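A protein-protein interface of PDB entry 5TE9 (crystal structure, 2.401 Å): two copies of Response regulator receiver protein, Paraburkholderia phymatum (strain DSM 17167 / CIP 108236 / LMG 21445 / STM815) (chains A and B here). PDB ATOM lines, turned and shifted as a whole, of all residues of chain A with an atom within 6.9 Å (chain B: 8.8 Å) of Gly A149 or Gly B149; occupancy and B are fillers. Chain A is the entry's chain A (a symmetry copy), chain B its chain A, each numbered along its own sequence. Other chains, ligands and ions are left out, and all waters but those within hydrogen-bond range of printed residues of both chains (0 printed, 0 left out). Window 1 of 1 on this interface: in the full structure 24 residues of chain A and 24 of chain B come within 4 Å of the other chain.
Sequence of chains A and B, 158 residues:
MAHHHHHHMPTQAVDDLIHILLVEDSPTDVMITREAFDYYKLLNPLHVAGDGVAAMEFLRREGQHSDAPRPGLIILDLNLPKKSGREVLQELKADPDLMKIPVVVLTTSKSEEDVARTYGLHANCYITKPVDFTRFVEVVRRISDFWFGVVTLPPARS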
ATOM      1  N   ASP A  16      -9.437 -11.818 -10.609  1.00  0.00           N
ATOM      2  CA  ASP A  16     -10.454 -12.650 -11.226  1.00  0.00           C
ATOM      3  C   ASP A  16     -10.006 -14.089 -11.253  1.00  0.00           C
ATOM      4  O   ASP A  16     -10.464 -14.855 -12.078  1.00  0.00           O
ATOM      5  CB  ASP A  16     -10.754 -12.183 -12.646  1.00  0.00           C
ATOM      6  N   LEU A  17      -9.108 -14.461 -10.345  1.00  0.00           N
ATOM      7  CA  LEU A  17      -8.607 -15.825 -10.381  1.00  0.00           C
ATOM      8  C   LEU A  17      -9.680 -16.830  -9.970  1.00  0.00           C
ATOM      9  O   LEU A  17      -9.765 -17.908 -10.565  1.00  0.00           O
ATOM     10  CB  LEU A  17      -7.351 -15.943  -9.518  1.00  0.00           C
ATOM     11  CG  LEU A  17      -6.100 -15.508 -10.300  1.00  0.00           C
ATOM     12  CD1 LEU A  17      -4.895 -15.265  -9.395  1.00  0.00           C
ATOM     13  CD2 LEU A  17      -5.760 -16.512 -11.413  1.00  0.00           C
ATOM     14  N   LYS A  41     -19.722  -7.217 -16.382  1.00  0.00           N
ATOM     15  CA  LYS A  41     -18.328  -7.463 -16.746  1.00  0.00           C
ATOM     16  C   LYS A  41     -17.551  -8.095 -15.601  1.00  0.00           C
ATOM     17  O   LYS A  41     -16.444  -7.671 -15.260  1.00  0.00           O
ATOM     18  CB  LYS A  41     -17.640  -6.176 -17.215  1.00  0.00           C
ATOM     19  CG  LYS A  41     -17.960  -5.778 -18.632  1.00  0.00           C
ATOM     20  CD  LYS A  41     -18.175  -4.271 -18.693  1.00  0.00           C
ATOM     21  CE  LYS A  41     -17.409  -3.617 -19.817  1.00  0.00           C
ATOM     22  NZ  LYS A  41     -15.953  -3.674 -19.627  1.00  0.00           N
ATOM     23  N   LEU A  42     -18.145  -9.111 -14.988  1.00  0.00           N
ATOM     24  CA  LEU A  42     -17.405  -9.928 -14.039  1.00  0.00           C
ATOM     25  C   LEU A  42     -16.557 -10.903 -14.823  1.00  0.00           C
ATOM     26  O   LEU A  42     -17.065 -11.622 -15.683  1.00  0.00           O
ATOM     27  CB  LEU A  42     -18.341 -10.683 -13.099  1.00  0.00           C
ATOM     28  CG  LEU A  42     -18.567 -10.009 -11.753  1.00  0.00           C
ATOM     29  CD1 LEU A  42     -19.771 -10.636 -11.100  1.00  0.00           C
ATOM     30  CD2 LEU A  42     -17.334 -10.156 -10.874  1.00  0.00           C
ATOM     31  N   LEU A  43     -15.267 -10.919 -14.541  1.00  0.00           N
ATOM     32  CA  LEU A  43     -14.400 -11.862 -15.218  1.00  0.00           C
ATOM     33  C   LEU A  43     -14.404 -13.243 -14.582  1.00  0.00           C
ATOM     34  O   LEU A  43     -13.878 -14.175 -15.192  1.00  0.00           O
ATOM     35  CB  LEU A  43     -12.974 -11.330 -15.259  1.00  0.00           C
ATOM     36  CG  LEU A  43     -12.738 -10.322 -16.388  1.00  0.00           C
ATOM     37  CD1 LEU A  43     -11.261 -10.013 -16.544  1.00  0.00           C
ATOM     38  CD2 LEU A  43     -13.311 -10.884 -17.675  1.00  0.00           C
ATOM     39  N   ASN A  44     -14.963 -13.396 -13.390  1.00  0.00           N
ATOM     40  CA  ASN A  44     -14.830 -14.651 -12.656  1.00  0.00           C
ATOM     41  C   ASN A  44     -15.602 -15.744 -13.386  1.00  0.00           C
ATOM     42  O   ASN A  44     -16.819 -15.608 -13.558  1.00  0.00           O
ATOM     43  CB  ASN A  44     -15.362 -14.497 -11.227  1.00  0.00           C
ATOM     44  CG  ASN A  44     -14.573 -13.508 -10.419  1.00  0.00           C
ATOM     45  OD1 ASN A  44     -14.907 -12.329 -10.360  1.00  0.00           O
ATOM     46  ND2 ASN A  44     -13.508 -13.978  -9.796  1.00  0.00           N
ATOM     47  N   TRP A 147     -12.566  -9.363  -2.445  1.00  0.00           N
ATOM     48  CA  TRP A 147     -12.471  -7.953  -2.797  1.00  0.00           C
ATOM     49  C   TRP A 147     -12.803  -7.758  -4.268  1.00  0.00           C
ATOM     50  O   TRP A 147     -12.551  -8.637  -5.095  1.00  0.00           O
ATOM     51  CB  TRP A 147     -11.076  -7.393  -2.535  1.00  0.00           C
ATOM     52  CG  TRP A 147     -10.633  -7.511  -1.134  1.00  0.00           C
ATOM     53  CD1 TRP A 147     -10.135  -8.630  -0.517  1.00  0.00           C
ATOM     54  CD2 TRP A 147     -10.618  -6.471  -0.158  1.00  0.00           C
ATOM     55  NE1 TRP A 147      -9.829  -8.349   0.789  1.00  0.00           N
ATOM     56  CE2 TRP A 147     -10.114  -7.032   1.037  1.00  0.00           C
ATOM     57  CE3 TRP A 147     -10.990  -5.124  -0.173  1.00  0.00           C
ATOM     58  CZ2 TRP A 147      -9.970  -6.294   2.195  1.00  0.00           C
ATOM     59  CZ3 TRP A 147     -10.854  -4.395   0.973  1.00  0.00           C
ATOM     60  CH2 TRP A 147     -10.340  -4.975   2.147  1.00  0.00           C
ATOM     61  N   PHE A 148     -13.362  -6.590  -4.588  1.00  0.00           N
ATOM     62  CA  PHE A 148     -13.537  -6.177  -5.969  1.00  0.00           C
ATOM     63  C   PHE A 148     -12.308  -5.432  -6.469  1.00  0.00           C
ATOM     64  O   PHE A 148     -11.750  -4.581  -5.773  1.00  0.00           O
ATOM     65  CB  PHE A 148     -14.756  -5.274  -6.121  1.00  0.00           C
ATOM     66  CG  PHE A 148     -16.045  -6.004  -6.161  1.00  0.00           C
ATOM     67  CD1 PHE A 148     -16.295  -6.935  -7.160  1.00  0.00           C
ATOM     68  CD2 PHE A 148     -17.024  -5.757  -5.218  1.00  0.00           C
ATOM     69  CE1 PHE A 148     -17.490  -7.603  -7.211  1.00  0.00           C
ATOM     70  CE2 PHE A 148     -18.229  -6.428  -5.268  1.00  0.00           C
ATOM     71  CZ  PHE A 148     -18.459  -7.354  -6.261  1.00  0.00           C
ATOM     72  N   GLY A 149     -11.909  -5.732  -7.697  1.00  0.00           N
ATOM     73  CA  GLY A 149     -10.913  -4.919  -8.354  1.00  0.00           C
ATOM     74  C   GLY A 149     -11.258  -4.647  -9.799  1.00  0.00           C
ATOM     75  O   GLY A 149     -11.791  -5.517 -10.485  1.00  0.00           O
ATOM     76  N   VAL A 150     -10.953  -3.456 -10.288  1.00  0.00           N
ATOM     77  CA  VAL A 150     -11.130  -3.142 -11.701  1.00  0.00           C
ATOM     78  C   VAL A 150      -9.827  -3.457 -12.417  1.00  0.00           C
ATOM     79  O   VAL A 150      -8.771  -2.930 -12.060  1.00  0.00           O
ATOM     80  CB  VAL A 150     -11.535  -1.678 -11.896  1.00  0.00           C
ATOM     81  CG1 VAL A 150     -11.724  -1.388 -13.352  1.00  0.00           C
ATOM     82  CG2 VAL A 150     -12.814  -1.386 -11.108  1.00  0.00           C
ATOM     83  N   VAL A 151      -9.892  -4.317 -13.422  1.00  0.00           N
ATOM     84  CA  VAL A 151      -8.704  -4.727 -14.153  1.00  0.00           C
ATOM     85  C   VAL A 151      -8.794  -4.251 -15.598  1.00  0.00           C
ATOM     86  O   VAL A 151      -9.838  -4.366 -16.252  1.00  0.00           O
ATOM     87  CB  VAL A 151      -8.505  -6.249 -14.084  1.00  0.00           C
ATOM     88  CG1 VAL A 151      -9.730  -6.963 -14.607  1.00  0.00           C
ATOM     89  CG2 VAL A 151      -7.271  -6.640 -14.868  1.00  0.00           C
ATOM     90  N   ASP B  16      -6.766  -5.349  -9.823  1.00  0.00           N
ATOM     91  CA  ASP B  16      -6.754  -4.122  -9.048  1.00  0.00           C
ATOM     92  C   ASP B  16      -5.475  -3.363  -9.292  1.00  0.00           C
ATOM     93  O   ASP B  16      -5.062  -2.579  -8.460  1.00  0.00           O
ATOM     94  CB  ASP B  16      -6.896  -4.415  -7.559  1.00  0.00           C
ATOM     95  N   LEU B  17      -4.844  -3.593 -10.440  1.00  0.00           N
ATOM     96  CA  LEU B  17      -3.575  -2.926 -10.682  1.00  0.00           C
ATOM     97  C   LEU B  17      -3.760  -1.426 -10.896  1.00  0.00           C
ATOM     98  O   LEU B  17      -2.942  -0.637 -10.417  1.00  0.00           O
ATOM     99  CB  LEU B  17      -2.853  -3.587 -11.856  1.00  0.00           C
ATOM    100  CG  LEU B  17      -2.066  -4.824 -11.394  1.00  0.00           C
ATOM    101  CD1 LEU B  17      -1.631  -5.714 -12.558  1.00  0.00           C
ATOM    102  CD2 LEU B  17      -0.863  -4.428 -10.524  1.00  0.00           C
ATOM    103  N   ILE B  18      -4.833  -0.998 -11.559  1.00  0.00           N
ATOM    104  CA  ILE B  18      -4.882   0.388 -12.030  1.00  0.00           C
ATOM    105  C   ILE B  18      -5.326   1.321 -10.909  1.00  0.00           C
ATOM    106  O   ILE B  18      -6.306   1.056 -10.194  1.00  0.00           O
ATOM    107  CB  ILE B  18      -5.775   0.544 -13.278  1.00  0.00           C
ATOM    108  CG1 ILE B  18      -7.229   0.186 -13.009  1.00  0.00           C
ATOM    109  CG2 ILE B  18      -5.225  -0.250 -14.440  1.00  0.00           C
ATOM    110  CD1 ILE B  18      -8.186   1.271 -13.474  1.00  0.00           C
ATOM    111  N   ILE B  20      -6.770   5.044  -9.656  1.00  0.00           N
ATOM    112  CA  ILE B  20      -7.843   5.925 -10.077  1.00  0.00           C
ATOM    113  C   ILE B  20      -7.553   7.320  -9.537  1.00  0.00           C
ATOM    114  O   ILE B  20      -7.247   7.477  -8.350  1.00  0.00           O
ATOM    115  CB  ILE B  20      -9.189   5.382  -9.579  1.00  0.00           C
ATOM    116  CG1 ILE B  20      -9.450   4.018 -10.218  1.00  0.00           C
ATOM    117  CG2 ILE B  20     -10.326   6.354  -9.869  1.00  0.00           C
ATOM    118  CD1 ILE B  20     -10.645   3.287  -9.647  1.00  0.00           C
ATOM    119  N   TYR B  40     -17.694  -1.025  -0.486  1.00  0.00           N
ATOM    120  CA  TYR B  40     -17.840  -2.106  -1.453  1.00  0.00           C
ATOM    121  C   TYR B  40     -16.521  -2.776  -1.804  1.00  0.00           C
ATOM    122  O   TYR B  40     -16.480  -3.583  -2.734  1.00  0.00           O
ATOM    123  CB  TYR B  40     -18.543  -1.599  -2.704  1.00  0.00           C
ATOM    124  CG  TYR B  40     -19.968  -1.221  -2.390  1.00  0.00           C
ATOM    125  CD1 TYR B  40     -20.968  -2.172  -2.360  1.00  0.00           C
ATOM    126  CD2 TYR B  40     -20.304   0.068  -2.084  1.00  0.00           C
ATOM    127  CE1 TYR B  40     -22.265  -1.834  -2.057  1.00  0.00           C
ATOM    128  CE2 TYR B  40     -21.593   0.417  -1.776  1.00  0.00           C
ATOM    129  CZ  TYR B  40     -22.573  -0.531  -1.770  1.00  0.00           C
ATOM    130  OH  TYR B  40     -23.861  -0.163  -1.460  1.00  0.00           O
ATOM    131  N   LYS B  41     -15.451  -2.481  -1.069  1.00  0.00           N
ATOM    132  CA  LYS B  41     -14.221  -3.269  -1.118  1.00  0.00           C
ATOM    133  C   LYS B  41     -13.564  -3.201  -2.488  1.00  0.00           C
ATOM    134  O   LYS B  41     -13.168  -4.217  -3.065  1.00  0.00           O
ATOM    135  CB  LYS B  41     -14.477  -4.726  -0.717  1.00  0.00           C
ATOM    136  CG  LYS B  41     -14.588  -4.954   0.768  1.00  0.00           C
ATOM    137  CD  LYS B  41     -15.726  -5.928   1.042  1.00  0.00           C
ATOM    138  CE  LYS B  41     -15.332  -7.039   1.983  1.00  0.00           C
ATOM    139  NZ  LYS B  41     -14.332  -7.950   1.407  1.00  0.00           N
ATOM    140  N   LEU B  42     -13.462  -1.992  -3.024  1.00  0.00           N
ATOM    141  CA  LEU B  42     -12.655  -1.784  -4.216  1.00  0.00           C
ATOM    142  C   LEU B  42     -11.206  -1.713  -3.793  1.00  0.00           C
ATOM    143  O   LEU B  42     -10.850  -0.934  -2.909  1.00  0.00           O
ATOM    144  CB  LEU B  42     -13.052  -0.504  -4.947  1.00  0.00           C
ATOM    145  CG  LEU B  42     -14.018  -0.708  -6.106  1.00  0.00           C
ATOM    146  CD1 LEU B  42     -14.611   0.626  -6.476  1.00  0.00           C
ATOM    147  CD2 LEU B  42     -13.296  -1.331  -7.291  1.00  0.00           C
ATOM    148  N   LEU B  43     -10.373  -2.533  -4.409  1.00  0.00           N
ATOM    149  CA  LEU B  43      -8.961  -2.487  -4.090  1.00  0.00           C
ATOM    150  C   LEU B  43      -8.211  -1.400  -4.843  1.00  0.00           C
ATOM    151  O   LEU B  43      -7.061  -1.128  -4.496  1.00  0.00           O
ATOM    152  CB  LEU B  43      -8.314  -3.836  -4.374  1.00  0.00           C
ATOM    153  CG  LEU B  43      -8.522  -4.855  -3.250  1.00  0.00           C
ATOM    154  CD1 LEU B  43      -7.659  -6.086  -3.461  1.00  0.00           C
ATOM    155  CD2 LEU B  43      -8.202  -4.193  -1.923  1.00  0.00           C
ATOM    156  N   ASN B  44      -8.815  -0.790  -5.852  1.00  0.00           N
ATOM    157  CA  ASN B  44      -8.080   0.124  -6.722  1.00  0.00           C
ATOM    158  C   ASN B  44      -7.693   1.368  -5.932  1.00  0.00           C
ATOM    159  O   ASN B  44      -8.584   2.063  -5.428  1.00  0.00           O
ATOM    160  CB  ASN B  44      -8.933   0.515  -7.934  1.00  0.00           C
ATOM    161  CG  ASN B  44      -9.260  -0.656  -8.814  1.00  0.00           C
ATOM    162  OD1 ASN B  44     -10.295  -1.295  -8.658  1.00  0.00           O
ATOM    163  ND2 ASN B  44      -8.372  -0.954  -9.744  1.00  0.00           N
ATOM    164  N   PRO B  45      -6.401   1.675  -5.781  1.00  0.00           N
ATOM    165  CA  PRO B  45      -6.010   2.915  -5.092  1.00  0.00           C
ATOM    166  C   PRO B  45      -6.740   4.118  -5.660  1.00  0.00           C
ATOM    167  O   PRO B  45      -6.697   4.364  -6.864  1.00  0.00           O
ATOM    168  CB  PRO B  45      -4.502   3.015  -5.350  1.00  0.00           C
ATOM    169  CG  PRO B  45      -4.066   1.629  -5.650  1.00  0.00           C
ATOM    170  CD  PRO B  45      -5.239   0.904  -6.258  1.00  0.00           C
ATOM    171  N   PHE B 133     -21.070   3.975  -5.761  1.00  0.00           N
ATOM    172  CA  PHE B 133     -20.623   2.706  -6.329  1.00  0.00           C
ATOM    173  C   PHE B 133     -21.428   2.341  -7.569  1.00  0.00           C
ATOM    174  O   PHE B 133     -20.875   1.816  -8.536  1.00  0.00           O
ATOM    175  CB  PHE B 133     -20.702   1.593  -5.282  1.00  0.00           C
ATOM    176  CG  PHE B 133     -20.175   0.266  -5.763  1.00  0.00           C
ATOM    177  CD1 PHE B 133     -18.818   0.090  -5.997  1.00  0.00           C
ATOM    178  CD2 PHE B 133     -21.028  -0.799  -5.965  1.00  0.00           C
ATOM    179  CE1 PHE B 133     -18.320  -1.126  -6.423  1.00  0.00           C
ATOM    180  CE2 PHE B 133     -20.545  -2.030  -6.403  1.00  0.00           C
ATOM    181  CZ  PHE B 133     -19.184  -2.188  -6.628  1.00  0.00           C
ATOM    182  N   PHE B 136     -20.085   4.326 -10.421  1.00  0.00           N
ATOM    183  CA  PHE B 136     -18.768   3.811 -10.766  1.00  0.00           C
ATOM    184  C   PHE B 136     -18.880   2.491 -11.506  1.00  0.00           C
ATOM    185  O   PHE B 136     -18.083   2.206 -12.408  1.00  0.00           O
ATOM    186  CB  PHE B 136     -17.911   3.640  -9.526  1.00  0.00           C
ATOM    187  CG  PHE B 136     -16.544   3.098  -9.817  1.00  0.00           C
ATOM    188  CD1 PHE B 136     -15.535   3.929 -10.278  1.00  0.00           C
ATOM    189  CD2 PHE B 136     -16.266   1.761  -9.637  1.00  0.00           C
ATOM    190  CE1 PHE B 136     -14.264   3.435 -10.545  1.00  0.00           C
ATOM    191  CE2 PHE B 136     -15.003   1.269  -9.902  1.00  0.00           C
ATOM    192  CZ  PHE B 136     -13.998   2.108 -10.347  1.00  0.00           C
ATOM    193  N   VAL B 140     -17.370   1.639 -15.328  1.00  0.00           N
ATOM    194  CA  VAL B 140     -16.662   0.433 -15.725  1.00  0.00           C
ATOM    195  C   VAL B 140     -17.361  -0.224 -16.918  1.00  0.00           C
ATOM    196  O   VAL B 140     -16.706  -0.674 -17.866  1.00  0.00           O
ATOM    197  CB  VAL B 140     -16.534  -0.509 -14.510  1.00  0.00           C
ATOM    198  CG1 VAL B 140     -16.150  -1.921 -14.936  1.00  0.00           C
ATOM    199  CG2 VAL B 140     -15.509   0.070 -13.511  1.00  0.00           C
ATOM    200  N   PHE B 146     -12.142  -2.164 -19.410  1.00  0.00           N
ATOM    201  CA  PHE B 146     -12.217  -2.307 -17.961  1.00  0.00           C
ATOM    202  C   PHE B 146     -13.145  -3.455 -17.579  1.00  0.00           C
ATOM    203  O   PHE B 146     -14.210  -3.623 -18.172  1.00  0.00           O
ATOM    204  CB  PHE B 146     -12.728  -1.029 -17.296  1.00  0.00           C
ATOM    205  CG  PHE B 146     -11.726   0.079 -17.241  1.00  0.00           C
ATOM    206  CD1 PHE B 146     -10.427  -0.124 -17.651  1.00  0.00           C
ATOM    207  CD2 PHE B 146     -12.093   1.323 -16.763  1.00  0.00           C
ATOM    208  CE1 PHE B 146      -9.510   0.903 -17.598  1.00  0.00           C
ATOM    209  CE2 PHE B 146     -11.187   2.357 -16.704  1.00  0.00           C
ATOM    210  CZ  PHE B 146      -9.889   2.152 -17.124  1.00  0.00           C
ATOM    211  N   TRP B 147     -12.756  -4.215 -16.554  1.00  0.00           N
ATOM    212  CA  TRP B 147     -13.538  -5.354 -16.095  1.00  0.00           C
ATOM    213  C   TRP B 147     -13.506  -5.431 -14.576  1.00  0.00           C
ATOM    214  O   TRP B 147     -12.524  -5.038 -13.943  1.00  0.00           O
ATOM    215  CB  TRP B 147     -13.011  -6.671 -16.659  1.00  0.00           C
ATOM    216  CG  TRP B 147     -12.997  -6.733 -18.131  1.00  0.00           C
ATOM    217  CD1 TRP B 147     -12.068  -6.175 -18.972  1.00  0.00           C
ATOM    218  CD2 TRP B 147     -13.940  -7.407 -18.961  1.00  0.00           C
ATOM    219  NE1 TRP B 147     -12.391  -6.450 -20.276  1.00  0.00           N
ATOM    220  CE2 TRP B 147     -13.534  -7.205 -20.300  1.00  0.00           C
ATOM    221  CE3 TRP B 147     -15.095  -8.154 -18.707  1.00  0.00           C
ATOM    222  CZ2 TRP B 147     -14.235  -7.723 -21.370  1.00  0.00           C
ATOM    223  CZ3 TRP B 147     -15.792  -8.661 -19.765  1.00  0.00           C
ATOM    224  CH2 TRP B 147     -15.360  -8.453 -21.087  1.00  0.00           C
ATOM    225  N   PHE B 148     -14.589  -5.952 -13.998  1.00  0.00           N
ATOM    226  CA  PHE B 148     -14.619  -6.284 -12.585  1.00  0.00           C
ATOM    227  C   PHE B 148     -14.128  -7.707 -12.355  1.00  0.00           C
ATOM    228  O   PHE B 148     -14.494  -8.633 -13.081  1.00  0.00           O
ATOM    229  CB  PHE B 148     -16.029  -6.152 -12.020  1.00  0.00           C
ATOM    230  CG  PHE B 148     -16.427  -4.758 -11.715  1.00  0.00           C
ATOM    231  CD1 PHE B 148     -15.713  -4.010 -10.789  1.00  0.00           C
ATOM    232  CD2 PHE B 148     -17.524  -4.188 -12.332  1.00  0.00           C
ATOM    233  CE1 PHE B 148     -16.085  -2.725 -10.492  1.00  0.00           C
ATOM    234  CE2 PHE B 148     -17.900  -2.894 -12.033  1.00  0.00           C
ATOM    235  CZ  PHE B 148     -17.177  -2.162 -11.118  1.00  0.00           C
ATOM    236  N   GLY B 149     -13.324  -7.880 -11.317  1.00  0.00           N
ATOM    237  CA  GLY B 149     -12.999  -9.214 -10.867  1.00  0.00           C
ATOM    238  C   GLY B 149     -13.035  -9.335  -9.362  1.00  0.00           C
ATOM    239  O   GLY B 149     -12.642  -8.410  -8.654  1.00  0.00           O
ATOM    240  N   VAL B 150     -13.488 -10.468  -8.849  1.00  0.00           N
ATOM    241  CA  VAL B 150     -13.444 -10.729  -7.416  1.00  0.00           C
ATOM    242  C   VAL B 150     -12.138 -11.442  -7.110  1.00  0.00           C
ATOM    243  O   VAL B 150     -11.850 -12.499  -7.678  1.00  0.00           O
ATOM    244  CB  VAL B 150     -14.651 -11.559  -6.968  1.00  0.00           C
ATOM    245  CG1 VAL B 150     -14.589 -11.799  -5.492  1.00  0.00           C
ATOM    246  CG2 VAL B 150     -15.946 -10.838  -7.351  1.00  0.00           C
ATOM    247  N   VAL B 151     -11.341 -10.870  -6.220  1.00  0.00           N
ATOM    248  CA  VAL B 151     -10.046 -11.438  -5.879  1.00  0.00           C
ATOM    249  C   VAL B 151     -10.042 -11.880  -4.421  1.00  0.00           C
ATOM    250  O   VAL B 151     -10.517 -11.167  -3.527  1.00  0.00           O
ATOM    251  CB  VAL B 151      -8.910 -10.442  -6.157  1.00  0.00           C
ATOM    252  CG1 VAL B 151      -9.146  -9.153  -5.405  1.00  0.00           C
ATOM    253  CG2 VAL B 151      -7.583 -11.059  -5.776  1.00  0.00           C
ATOM    254  N   THR B 152      -9.515 -13.069  -4.188  1.00  0.00           N
ATOM    255  CA  THR B 152      -9.318 -13.531  -2.833  1.00  0.00           C
ATOM    256  C   THR B 152      -7.998 -12.976  -2.310  1.00  0.00           C
ATOM    257  O   THR B 152      -7.054 -12.739  -3.067  1.00  0.00           O
ATOM    258  CB  THR B 152      -9.354 -15.060  -2.784  1.00  0.00           C
ATOM    259  OG1 THR B 152      -9.316 -15.501  -1.424  1.00  0.00           O
ATOM    260  CG2 THR B 152      -8.186 -15.659  -3.554  1.00  0.00           C
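Among the printed residues, pairs that only touch across the chains: Trp A147 with Val B150, Val A150 with Trp B147, Phe A148 with Leu B42, Leu A42 with Phe B148, Phe A148 with Tyr B40, Leu A43 with Trp B147, Trp A147 with Leu B43, Trp A147 with Lys B41, Lys A41 with Trp B147, Lys A41 with Val B140, Gly A149 with Trp B147, Trp A147 with Gly B149, Val A151 with Phe B146, Phe A148 with Val B150, Val A150 with Phe B148, Val A150 with Ile B18, Gly A149 with Phe B148, Phe A148 with Gly B149, Val A150 with Phe B136, Asn A44 with Gly B149, Gly A149 with Asn B44, Asp A16 with Val B150, Val A150 with Asp B16, Leu A42 with Val B150, Val A150 with Leu B42 and Val A150 with Val B140.
Of chain B, only Asn B44 (3.7 Å), Trp B147 (3.6 Å), Phe B148 (3.6 Å) and Gly B149 (2.9 Å) come within 4 Å of Gly A149.
Of the printed residues of chain A, Gly B149 touches Asn A44 (3.7 Å), Trp A147 (3.6 Å), Phe A148 (3.6 Å) and Gly A149 (2.9 Å).
Printed residues of chain B within 4 Å of Asp A16: Val B150 (3.8 Å).
Printed residues of chain A within 4 Å of Tyr B40: Phe A148.
Of the printed residues of chain B, Phe A148 touches Tyr B40, Lys B41, Leu B42, Leu B43, Gly B149 and Val B150.
Of the printed residues of chain A, Val B151 touches Trp A147 (2.8 Å).
Phe B133 touches none of the printed residues of chain A.
Leu A17 touches none of the printed residues of chain B.
The nearest residue of chain A that does not touch Gly B149 is Asp A16 (4.1 Å).
ND2 of Asn B44 lies within hydrogen-bond range of O of Ile B18 (2.9 Å).
Of the 20 printed residues of chain B, 15 touch a printed residue of chain A.
Printed residues of chain B that touch a printed residue of chain A: Asp B16, Ile B18, Tyr B40, Lys B41, Leu B42, Leu B43, Asn B44, Phe B136, Val B140, Phe B146, Trp B147, Phe B148, Gly B149, Val B150 and Val B151.
Hydrophobic or aromatic side chains of chain B that line the printed part of chain A: Ile B18, Leu B42, Leu B43, Phe B136, Val B140, Trp B147, Phe B148, Val B150 and Val B151.
Along chain B the printed residues that touch a printed residue of chain A span positions 16 to 151.
Of the 11 printed residues of chain A, 10 touch a printed residue of chain B.
Printed residues of chain A that touch a printed residue of chain B: Asp A16, Lys A41, Leu A42, Leu A43, Asn A44, Trp A147, Phe A148, Gly A149, Val A150 and Val A151.
Hydrophobic or aromatic side chains of chain A within 4 Å of the printed part of chain B: Leu A42, Leu A43, Trp A147, Phe A148, Val A150 and Val A151.
Along chain A the printed residues that touch a printed residue of chain B span positions 16 to 151.
N of Phe A148 sits at hydrogen-bond distance from O of Lys B41, 2.8 Å away.
The backbone NH (N) of Leu B43 lies within hydrogen-bond range of the backbone carbonyl oxygen (O) of Phe A148 (2.8 Å).
N of Val A150 lies within hydrogen-bond range of OD1 of Asn B44 (2.8 Å).
The backbone carbonyl oxygen (O) of Trp B147 is in hydrogen-bond range of the backbone NH (N) of Val A151.
The backbone carbonyl oxygen (O) of Lys A41 lies within hydrogen-bond range of the backbone NH (N) of Phe B148, at 2.8 Å.
The backbone NH (N) of Leu A43 lies within hydrogen-bond range of the backbone carbonyl oxygen (O) of Phe B148, at 2.8 Å.
N of Gly B149 is in hydrogen-bond range of O of Gly A149, 2.9 Å away.
The side-chain amide oxygen of Asn A44 is in hydrogen-bond range of the backbone NH of Val B150.
The backbone NH of Val B151 lies within hydrogen-bond range of the backbone carbonyl oxygen of Trp A147 (2.8 Å).
The side-chain amino group (NZ) of Lys A41 sits close to the backbone carbonyl oxygen (O) of Phe B146 (2.3 Å).
Lys A41 touches Phe B148, and with the chains exchanged Phe A148 touches Lys B41.
Asn A44 touches Val B150, and with the chains exchanged Val A150 touches Asn B44.
Trp A147 touches Gly B149, and with the chains exchanged Gly A149 touches Trp B147.
Trp A147 touches Val B151, and with the chains exchanged Val A151 touches Trp B147.
11 positions are printed for both chains.
Of the 36 pairs that touch across the chains among the printed residues, 29 have their exchanged pair printed and touching as well.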
